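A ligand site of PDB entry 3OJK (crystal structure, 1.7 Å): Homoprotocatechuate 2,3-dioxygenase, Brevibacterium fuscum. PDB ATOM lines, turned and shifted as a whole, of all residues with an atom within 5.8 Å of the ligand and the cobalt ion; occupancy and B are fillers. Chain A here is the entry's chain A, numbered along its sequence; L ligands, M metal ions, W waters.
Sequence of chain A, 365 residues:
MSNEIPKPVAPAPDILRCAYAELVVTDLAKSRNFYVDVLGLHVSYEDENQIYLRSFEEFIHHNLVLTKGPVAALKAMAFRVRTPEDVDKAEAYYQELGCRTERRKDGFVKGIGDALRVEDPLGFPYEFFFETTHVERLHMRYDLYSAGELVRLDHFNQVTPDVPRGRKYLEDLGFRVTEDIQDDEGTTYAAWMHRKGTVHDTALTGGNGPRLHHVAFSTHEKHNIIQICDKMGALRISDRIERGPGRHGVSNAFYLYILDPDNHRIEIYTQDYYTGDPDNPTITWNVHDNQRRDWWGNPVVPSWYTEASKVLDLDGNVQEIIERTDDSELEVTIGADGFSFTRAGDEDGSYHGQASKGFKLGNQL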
ATOM      1  N   HIS A 155     -29.515  16.160 -25.147  1.00  0.00           N
ATOM      2  CA  HIS A 155     -29.670  15.055 -24.166  1.00  0.00           C
ATOM      3  C   HIS A 155     -28.350  14.406 -23.755  1.00  0.00           C
ATOM      4  O   HIS A 155     -27.321  14.623 -24.377  1.00  0.00           O
ATOM      5  CB  HIS A 155     -30.611  13.991 -24.710  1.00  0.00           C
ATOM      6  CG  HIS A 155     -30.110  13.276 -25.930  1.00  0.00           C
ATOM      7  ND1 HIS A 155     -30.419  13.689 -27.206  1.00  0.00           N
ATOM      8  CD2 HIS A 155     -29.330  12.178 -26.067  1.00  0.00           C
ATOM      9  CE1 HIS A 155     -29.869  12.849 -28.084  1.00  0.00           C
ATOM     10  NE2 HIS A 155     -29.216  11.908 -27.420  1.00  0.00           N
ATOM     11  N   PHE A 156     -28.416  13.604 -22.696  1.00  0.00           N
ATOM     12  CA  PHE A 156     -27.392  12.661 -22.333  1.00  0.00           C
ATOM     13  C   PHE A 156     -27.906  11.238 -22.581  1.00  0.00           C
ATOM     14  O   PHE A 156     -29.125  11.013 -22.740  1.00  0.00           O
ATOM     15  CB  PHE A 156     -27.115  12.755 -20.837  1.00  0.00           C
ATOM     16  CG  PHE A 156     -26.910  14.161 -20.322  1.00  0.00           C
ATOM     17  CD1 PHE A 156     -25.938  14.982 -20.865  1.00  0.00           C
ATOM     18  CD2 PHE A 156     -27.660  14.630 -19.251  1.00  0.00           C
ATOM     19  CE1 PHE A 156     -25.744  16.270 -20.349  1.00  0.00           C
ATOM     20  CE2 PHE A 156     -27.460  15.915 -18.742  1.00  0.00           C
ATOM     21  CZ  PHE A 156     -26.515  16.724 -19.306  1.00  0.00           C
ATOM     22  N   ASN A 157     -26.998  10.275 -22.673  1.00  0.00           N
ATOM     23  CA  ASN A 157     -27.416   8.867 -22.695  1.00  0.00           C
ATOM     24  C   ASN A 157     -26.473   8.086 -21.772  1.00  0.00           C
ATOM     25  O   ASN A 157     -25.246   8.188 -21.887  1.00  0.00           O
ATOM     26  CB  ASN A 157     -27.420   8.353 -24.131  1.00  0.00           C
ATOM     27  CG  ASN A 157     -27.942   6.961 -24.256  1.00  0.00           C
ATOM     28  OD1 ASN A 157     -27.432   6.040 -23.662  1.00  0.00           O
ATOM     29  ND2 ASN A 157     -28.984   6.797 -25.060  1.00  0.00           N
ATOM     30  N   ILE A 181     -37.119   0.086 -26.078  1.00  0.00           N
ATOM     31  CA  ILE A 181     -36.827  -1.128 -26.829  1.00  0.00           C
ATOM     32  C   ILE A 181     -36.946  -2.341 -25.906  1.00  0.00           C
ATOM     33  O   ILE A 181     -36.325  -2.382 -24.831  1.00  0.00           O
ATOM     34  CB  ILE A 181     -35.414  -1.088 -27.455  1.00  0.00           C
ATOM     35  CG1 ILE A 181     -35.312   0.089 -28.425  1.00  0.00           C
ATOM     36  CG2 ILE A 181     -35.125  -2.461 -28.169  1.00  0.00           C
ATOM     37  CD1 ILE A 181     -33.886   0.250 -29.066  1.00  0.00           C
ATOM     38  N   TRP A 192     -36.012   5.984 -23.224  1.00  0.00           N
ATOM     39  CA  TRP A 192     -35.791   7.392 -23.414  1.00  0.00           C
ATOM     40  C   TRP A 192     -36.837   8.121 -22.610  1.00  0.00           C
ATOM     41  O   TRP A 192     -38.006   7.697 -22.597  1.00  0.00           O
ATOM     42  CB  TRP A 192     -36.000   7.713 -24.904  1.00  0.00           C
ATOM     43  CG  TRP A 192     -34.884   7.268 -25.811  1.00  0.00           C
ATOM     44  CD1 TRP A 192     -33.949   8.087 -26.389  1.00  0.00           C
ATOM     45  CD2 TRP A 192     -34.599   5.952 -26.294  1.00  0.00           C
ATOM     46  NE1 TRP A 192     -33.092   7.367 -27.161  1.00  0.00           N
ATOM     47  CE2 TRP A 192     -33.459   6.056 -27.126  1.00  0.00           C
ATOM     48  CE3 TRP A 192     -35.196   4.698 -26.127  1.00  0.00           C
ATOM     49  CZ2 TRP A 192     -32.895   4.947 -27.772  1.00  0.00           C
ATOM     50  CZ3 TRP A 192     -34.621   3.592 -26.763  1.00  0.00           C
ATOM     51  CH2 TRP A 192     -33.483   3.730 -27.580  1.00  0.00           C
ATOM     52  N   HIS A 200     -36.191  13.220 -25.442  1.00  0.00           N
ATOM     53  CA  HIS A 200     -35.501  12.968 -24.203  1.00  0.00           C
ATOM     54  C   HIS A 200     -34.576  14.087 -23.722  1.00  0.00           C
ATOM     55  O   HIS A 200     -34.112  14.942 -24.498  1.00  0.00           O
ATOM     56  CB  HIS A 200     -34.744  11.628 -24.237  1.00  0.00           C
ATOM     57  CG  HIS A 200     -33.734  11.467 -25.340  1.00  0.00           C
ATOM     58  ND1 HIS A 200     -33.993  11.793 -26.653  1.00  0.00           N
ATOM     59  CD2 HIS A 200     -32.514  10.896 -25.331  1.00  0.00           C
ATOM     60  CE1 HIS A 200     -32.943  11.468 -27.394  1.00  0.00           C
ATOM     61  NE2 HIS A 200     -32.037  10.918 -26.614  1.00  0.00           N
ATOM     62  N   HIS A 214     -23.174   8.892 -24.382  1.00  0.00           N
ATOM     63  CA  HIS A 214     -22.906  10.111 -25.127  1.00  0.00           C
ATOM     64  C   HIS A 214     -23.589  11.352 -24.568  1.00  0.00           C
ATOM     65  O   HIS A 214     -24.479  11.253 -23.743  1.00  0.00           O
ATOM     66  CB  HIS A 214     -23.283   9.906 -26.609  1.00  0.00           C
ATOM     67  CG  HIS A 214     -24.734   9.611 -26.876  1.00  0.00           C
ATOM     68  ND1 HIS A 214     -25.233   8.327 -26.959  1.00  0.00           N
ATOM     69  CD2 HIS A 214     -25.764  10.430 -27.187  1.00  0.00           C
ATOM     70  CE1 HIS A 214     -26.510   8.367 -27.277  1.00  0.00           C
ATOM     71  NE2 HIS A 214     -26.863   9.631 -27.419  1.00  0.00           N
ATOM     72  N   ALA A 216     -25.403  14.788 -26.478  1.00  0.00           N
ATOM     73  CA  ALA A 216     -25.932  15.081 -27.807  1.00  0.00           C
ATOM     74  C   ALA A 216     -26.251  16.559 -27.947  1.00  0.00           C
ATOM     75  O   ALA A 216     -26.885  17.160 -27.038  1.00  0.00           O
ATOM     76  CB  ALA A 216     -27.194  14.221 -28.085  1.00  0.00           C
ATOM     77  N   ARG A 243     -20.428   6.240 -36.300  1.00  0.00           N
ATOM     78  CA  ARG A 243     -21.681   5.693 -36.762  1.00  0.00           C
ATOM     79  C   ARG A 243     -22.514   6.794 -37.381  1.00  0.00           C
ATOM     80  O   ARG A 243     -22.621   7.890 -36.826  1.00  0.00           O
ATOM     81  CB  ARG A 243     -22.434   5.044 -35.593  1.00  0.00           C
ATOM     82  CG  ARG A 243     -23.776   4.498 -35.941  1.00  0.00           C
ATOM     83  CD  ARG A 243     -24.492   3.767 -34.794  1.00  0.00           C
ATOM     84  NE  ARG A 243     -25.887   3.674 -35.192  1.00  0.00           N
ATOM     85  CZ  ARG A 243     -26.940   3.854 -34.417  1.00  0.00           C
ATOM     86  NH1 ARG A 243     -26.842   3.997 -33.091  1.00  0.00           N
ATOM     87  NH2 ARG A 243     -28.144   3.839 -34.973  1.00  0.00           N
ATOM     88  N   HIS A 248     -32.755   7.978 -37.085  1.00  0.00           N
ATOM     89  CA  HIS A 248     -33.106   7.033 -36.018  1.00  0.00           C
ATOM     90  C   HIS A 248     -34.529   6.500 -36.263  1.00  0.00           C
ATOM     91  O   HIS A 248     -35.399   7.203 -36.808  1.00  0.00           O
ATOM     92  CB  HIS A 248     -33.099   7.734 -34.671  1.00  0.00           C
ATOM     93  CG  HIS A 248     -31.744   7.930 -34.065  1.00  0.00           C
ATOM     94  ND1 HIS A 248     -30.807   6.911 -33.955  1.00  0.00           N
ATOM     95  CD2 HIS A 248     -31.191   9.025 -33.486  1.00  0.00           C
ATOM     96  CE1 HIS A 248     -29.732   7.389 -33.354  1.00  0.00           C
ATOM     97  NE2 HIS A 248     -29.950   8.662 -33.048  1.00  0.00           N
ATOM     98  N   GLY A 249     -34.788   5.264 -35.856  1.00  0.00           N
ATOM     99  CA  GLY A 249     -36.162   4.828 -35.665  1.00  0.00           C
ATOM    100  C   GLY A 249     -36.740   5.453 -34.430  1.00  0.00           C
ATOM    101  O   GLY A 249     -37.611   6.303 -34.505  1.00  0.00           O
ATOM    102  N   VAL A 250     -36.270   4.971 -33.290  1.00  0.00           N
ATOM    103  CA  VAL A 250     -36.595   5.602 -32.032  1.00  0.00           C
ATOM    104  C   VAL A 250     -36.195   7.078 -32.107  1.00  0.00           C
ATOM    105  O   VAL A 250     -35.060   7.387 -32.492  1.00  0.00           O
ATOM    106  CB  VAL A 250     -35.798   4.981 -30.849  1.00  0.00           C
ATOM    107  CG1 VAL A 250     -36.042   5.860 -29.600  1.00  0.00           C
ATOM    108  CG2 VAL A 250     -36.184   3.503 -30.592  1.00  0.00           C
ATOM    109  N   SER A 251     -37.136   7.967 -31.823  1.00  0.00           N
ATOM    110  CA  SER A 251     -36.930   9.455 -31.829  1.00  0.00           C
ATOM    111  C   SER A 251     -37.169  10.114 -33.166  1.00  0.00           C
ATOM    112  O   SER A 251     -37.457  11.306 -33.222  1.00  0.00           O
ATOM    113  CB  SER A 251     -35.579   9.929 -31.307  1.00  0.00           C
ATOM    114  OG  SER A 251     -34.561   9.887 -32.287  1.00  0.00           O
ATOM    115  N   TYR A 257     -22.819  10.015 -34.874  1.00  0.00           N
ATOM    116  CA  TYR A 257     -21.959   9.790 -33.697  1.00  0.00           C
ATOM    117  C   TYR A 257     -20.494   9.930 -34.069  1.00  0.00           C
ATOM    118  O   TYR A 257     -19.981   9.228 -34.985  1.00  0.00           O
ATOM    119  CB  TYR A 257     -22.171   8.410 -33.084  1.00  0.00           C
ATOM    120  CG  TYR A 257     -23.563   8.157 -32.591  1.00  0.00           C
ATOM    121  CD1 TYR A 257     -23.978   8.593 -31.351  1.00  0.00           C
ATOM    122  CD2 TYR A 257     -24.476   7.488 -33.385  1.00  0.00           C
ATOM    123  CE1 TYR A 257     -25.266   8.383 -30.903  1.00  0.00           C
ATOM    124  CE2 TYR A 257     -25.774   7.250 -32.951  1.00  0.00           C
ATOM    125  CZ  TYR A 257     -26.159   7.720 -31.722  1.00  0.00           C
ATOM    126  OH  TYR A 257     -27.406   7.456 -31.274  1.00  0.00           O
ATOM    127  N   GLU A 267     -23.034  12.913 -29.943  1.00  0.00           N
ATOM    128  CA  GLU A 267     -24.039  12.792 -31.010  1.00  0.00           C
ATOM    129  C   GLU A 267     -24.428  14.162 -31.504  1.00  0.00           C
ATOM    130  O   GLU A 267     -24.562  15.090 -30.705  1.00  0.00           O
ATOM    131  CB  GLU A 267     -25.270  12.044 -30.494  1.00  0.00           C
ATOM    132  CG  GLU A 267     -26.295  11.694 -31.586  1.00  0.00           C
ATOM    133  CD  GLU A 267     -27.553  11.055 -31.034  1.00  0.00           C
ATOM    134  OE1 GLU A 267     -27.757  11.162 -29.808  1.00  0.00           O
ATOM    135  OE2 GLU A 267     -28.363  10.488 -31.822  1.00  0.00           O
ATOM    136  N   TYR A 269     -27.652  15.693 -33.544  1.00  0.00           N
ATOM    137  CA  TYR A 269     -29.024  15.219 -33.522  1.00  0.00           C
ATOM    138  C   TYR A 269     -29.944  16.325 -34.041  1.00  0.00           C
ATOM    139  O   TYR A 269     -29.659  17.512 -33.814  1.00  0.00           O
ATOM    140  CB  TYR A 269     -29.294  14.823 -32.059  1.00  0.00           C
ATOM    141  CG  TYR A 269     -30.617  14.288 -31.659  1.00  0.00           C
ATOM    142  CD1 TYR A 269     -30.848  12.923 -31.591  1.00  0.00           C
ATOM    143  CD2 TYR A 269     -31.632  15.149 -31.237  1.00  0.00           C
ATOM    144  CE1 TYR A 269     -32.043  12.408 -31.135  1.00  0.00           C
ATOM    145  CE2 TYR A 269     -32.860  14.636 -30.799  1.00  0.00           C
ATOM    146  CZ  TYR A 269     -33.033  13.256 -30.728  1.00  0.00           C
ATOM    147  OH  TYR A 269     -34.197  12.759 -30.236  1.00  0.00           O
ATOM    148  N   ARG A 292     -35.045  -0.047 -35.973  1.00  0.00           N
ATOM    149  CA  ARG A 292     -35.262   0.655 -34.695  1.00  0.00           C
ATOM    150  C   ARG A 292     -34.174   1.682 -34.326  1.00  0.00           C
ATOM    151  O   ARG A 292     -34.468   2.700 -33.707  1.00  0.00           O
ATOM    152  CB  ARG A 292     -35.364  -0.333 -33.522  1.00  0.00           C
ATOM    153  CG  ARG A 292     -34.014  -0.851 -33.070  1.00  0.00           C
ATOM    154  CD  ARG A 292     -34.106  -2.120 -32.229  1.00  0.00           C
ATOM    155  NE  ARG A 292     -32.726  -2.475 -31.890  1.00  0.00           N
ATOM    156  CZ  ARG A 292     -31.856  -3.047 -32.730  1.00  0.00           C
ATOM    157  NH1 ARG A 292     -32.244  -3.408 -33.956  1.00  0.00           N
ATOM    158  NH2 ARG A 292     -30.601  -3.285 -32.364  1.00  0.00           N
ATOM    159  N   ARG A 293     -32.933   1.428 -34.702  1.00  0.00           N
ATOM    160  CA  ARG A 293     -31.860   2.333 -34.347  1.00  0.00           C
ATOM    161  C   ARG A 293     -31.473   3.199 -35.523  1.00  0.00           C
ATOM    162  O   ARG A 293     -31.347   4.410 -35.382  1.00  0.00           O
ATOM    163  CB  ARG A 293     -30.667   1.578 -33.792  1.00  0.00           C
ATOM    164  CG  ARG A 293     -30.987   0.986 -32.393  1.00  0.00           C
ATOM    165  CD  ARG A 293     -29.746   0.888 -31.553  1.00  0.00           C
ATOM    166  NE  ARG A 293     -30.048   0.463 -30.166  1.00  0.00           N
ATOM    167  CZ  ARG A 293     -30.260   1.287 -29.137  1.00  0.00           C
ATOM    168  NH1 ARG A 293     -30.258   2.596 -29.286  1.00  0.00           N
ATOM    169  NH2 ARG A 293     -30.466   0.774 -27.927  1.00  0.00           N
ATOM    170  N   ASP A 294     -31.306   2.555 -36.670  1.00  0.00           N
ATOM    171  CA  ASP A 294     -31.169   3.222 -37.941  1.00  0.00           C
ATOM    172  C   ASP A 294     -32.334   2.816 -38.821  1.00  0.00           C
ATOM    173  O   ASP A 294     -32.448   1.640 -39.230  1.00  0.00           O
ATOM    174  CB  ASP A 294     -29.851   2.849 -38.641  1.00  0.00           C
ATOM    175  CG  ASP A 294     -29.592   3.729 -39.858  1.00  0.00           C
ATOM    176  OD1 ASP A 294     -29.916   3.293 -40.985  1.00  0.00           O
ATOM    177  OD2 ASP A 294     -29.160   4.870 -39.647  1.00  0.00           O
ATOM    178  N   TRP A 304     -20.349   0.734 -30.845  1.00  0.00           N
ATOM    179  CA  TRP A 304     -21.410   1.584 -30.321  1.00  0.00           C
ATOM    180  C   TRP A 304     -22.104   0.931 -29.110  1.00  0.00           C
ATOM    181  O   TRP A 304     -22.553   1.626 -28.188  1.00  0.00           O
ATOM    182  CB  TRP A 304     -22.414   1.898 -31.465  1.00  0.00           C
ATOM    183  CG  TRP A 304     -23.323   3.009 -31.157  1.00  0.00           C
ATOM    184  CD1 TRP A 304     -23.119   4.334 -31.448  1.00  0.00           C
ATOM    185  CD2 TRP A 304     -24.553   2.933 -30.461  1.00  0.00           C
ATOM    186  NE1 TRP A 304     -24.155   5.074 -30.990  1.00  0.00           N
ATOM    187  CE2 TRP A 304     -25.066   4.250 -30.375  1.00  0.00           C
ATOM    188  CE3 TRP A 304     -25.302   1.886 -29.928  1.00  0.00           C
ATOM    189  CZ2 TRP A 304     -26.286   4.546 -29.768  1.00  0.00           C
ATOM    190  CZ3 TRP A 304     -26.521   2.171 -29.331  1.00  0.00           C
ATOM    191  CH2 TRP A 304     -26.994   3.510 -29.243  1.00  0.00           C
HETATM  192  C1  LIG L   1     -30.943   8.745 -29.743  1.00  0.00           C
HETATM  193  C2  LIG L   1     -29.846   7.764 -29.709  1.00  0.00           C
HETATM  194  C3  LIG L   1     -30.069   6.494 -30.217  1.00  0.00           C
HETATM  195  C4  LIG L   1     -31.310   6.157 -30.740  1.00  0.00           C
HETATM  196  C5  LIG L   1     -32.350   7.096 -30.763  1.00  0.00           C
HETATM  197  C6  LIG L   1     -32.173   8.387 -30.262  1.00  0.00           C
HETATM  198  O1  LIG L   1     -30.691   9.994 -29.273  1.00  0.00           O
HETATM  199  O2  LIG L   1     -28.658   8.163 -29.229  1.00  0.00           O
HETATM  200  N1  LIG L   1     -31.478   4.906 -31.230  1.00  0.00           N
HETATM  201  O3  LIG L   1     -30.213   4.289 -31.912  1.00  0.00           O
HETATM  202  O4  LIG L   1     -32.524   4.877 -32.099  1.00  0.00           O
HETATM  203 CO    CO M   1     -28.732  10.042 -28.318  1.00  0.00          CO
HETATM  204  O   HOH W   1     -29.940   8.955 -26.607  1.00  0.00           O
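OH of Tyr 257 sits close to O2 of the ligand, at 2.5 Å.
The guanidinium group (NH1) of Arg 293 sits at hydrogen-bond distance from an oxygen (O3) of the ligand (3.1 Å).
NE2 of His 200 sits close to O1 of the ligand.
A ring nitrogen (ND1) of His 248 sits at hydrogen-bond distance from an oxygen (O4) of the ligand, 3.2 Å away.
The cobalt ion is bound by O2 of the ligand (2.1 Å).
The cobalt ion is bound by OE1 of Glu 267.
NE2 of His 214 is bound to the cobalt ion (2.1 Å).
The cobalt ion is bound by NE2 of His 155 (2.1 Å).
O1 of the ligand is bound to the cobalt ion (2.2 Å).
Water W1 binds the cobalt ion (2.4 Å).
The cobalt ion has six donor atoms within binding distance.
O of Arg 292 lies close to O4 of the ligand (3.3 Å).
NE1 of Trp 192 touches C6 of the ligand, 3.4 Å away.
Arg 243 touches the ligand.
O of Val 250 touches C5 of the ligand, at 3.2 Å.
Ser 251 touches the ligand.
CE1 of Tyr 269 touches O1 of the ligand, at 3.3 Å.
Hydrophobic or aromatic side chains within 4 Å of the ligand: His 155, Trp 192, His 200, His 214, His 248, Val 250, Tyr 257 and Tyr 269.
Within 4 Å of the ligand: His 155, Trp 192, His 200, His 214, Arg 243, His 248, Val 250, Ser 251, Tyr 257, Glu 267, Tyr 269, Arg 292 and Arg 293.
The nearest printed residue that does not touch the ligand is Trp 304 (4.3 Å).
Water W1 bridges ND2 of Asn 157 (2.8 Å) and NE2 of His 200 (2.9 Å).
Residues that only touch the cobalt ion: His 200.
Four residues have an atom within 4 Å of the cobalt ion: His 155, His 200, His 214 and Glu 267.
The side-chain carboxylate (OE2) of Glu 267 sits at hydrogen-bond distance from a ring nitrogen (NE2) of His 248 (2.7 Å).
The backbone carbonyl oxygen (O) of Arg 243 sits at hydrogen-bond distance from the backbone NH (N) of Tyr 257 (2.9 Å).
A ring nitrogen (NE2) of His 248 sits close to the side-chain hydroxyl of Tyr 257.
O of Arg 293 sits at hydrogen-bond distance from NH2 of Arg 243 (3.3 Å).
N of Ala 216 lies within hydrogen-bond range of O of His 155.
ND1 of His 155 lies close to NE2 of His 200, at 3.3 Å.
ND1 of His 248 sits at hydrogen-bond distance from O of Arg 293 (2.9 Å).
OE2 of Glu 267 is in hydrogen-bond range of OH of Tyr 257, 3.2 Å away.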
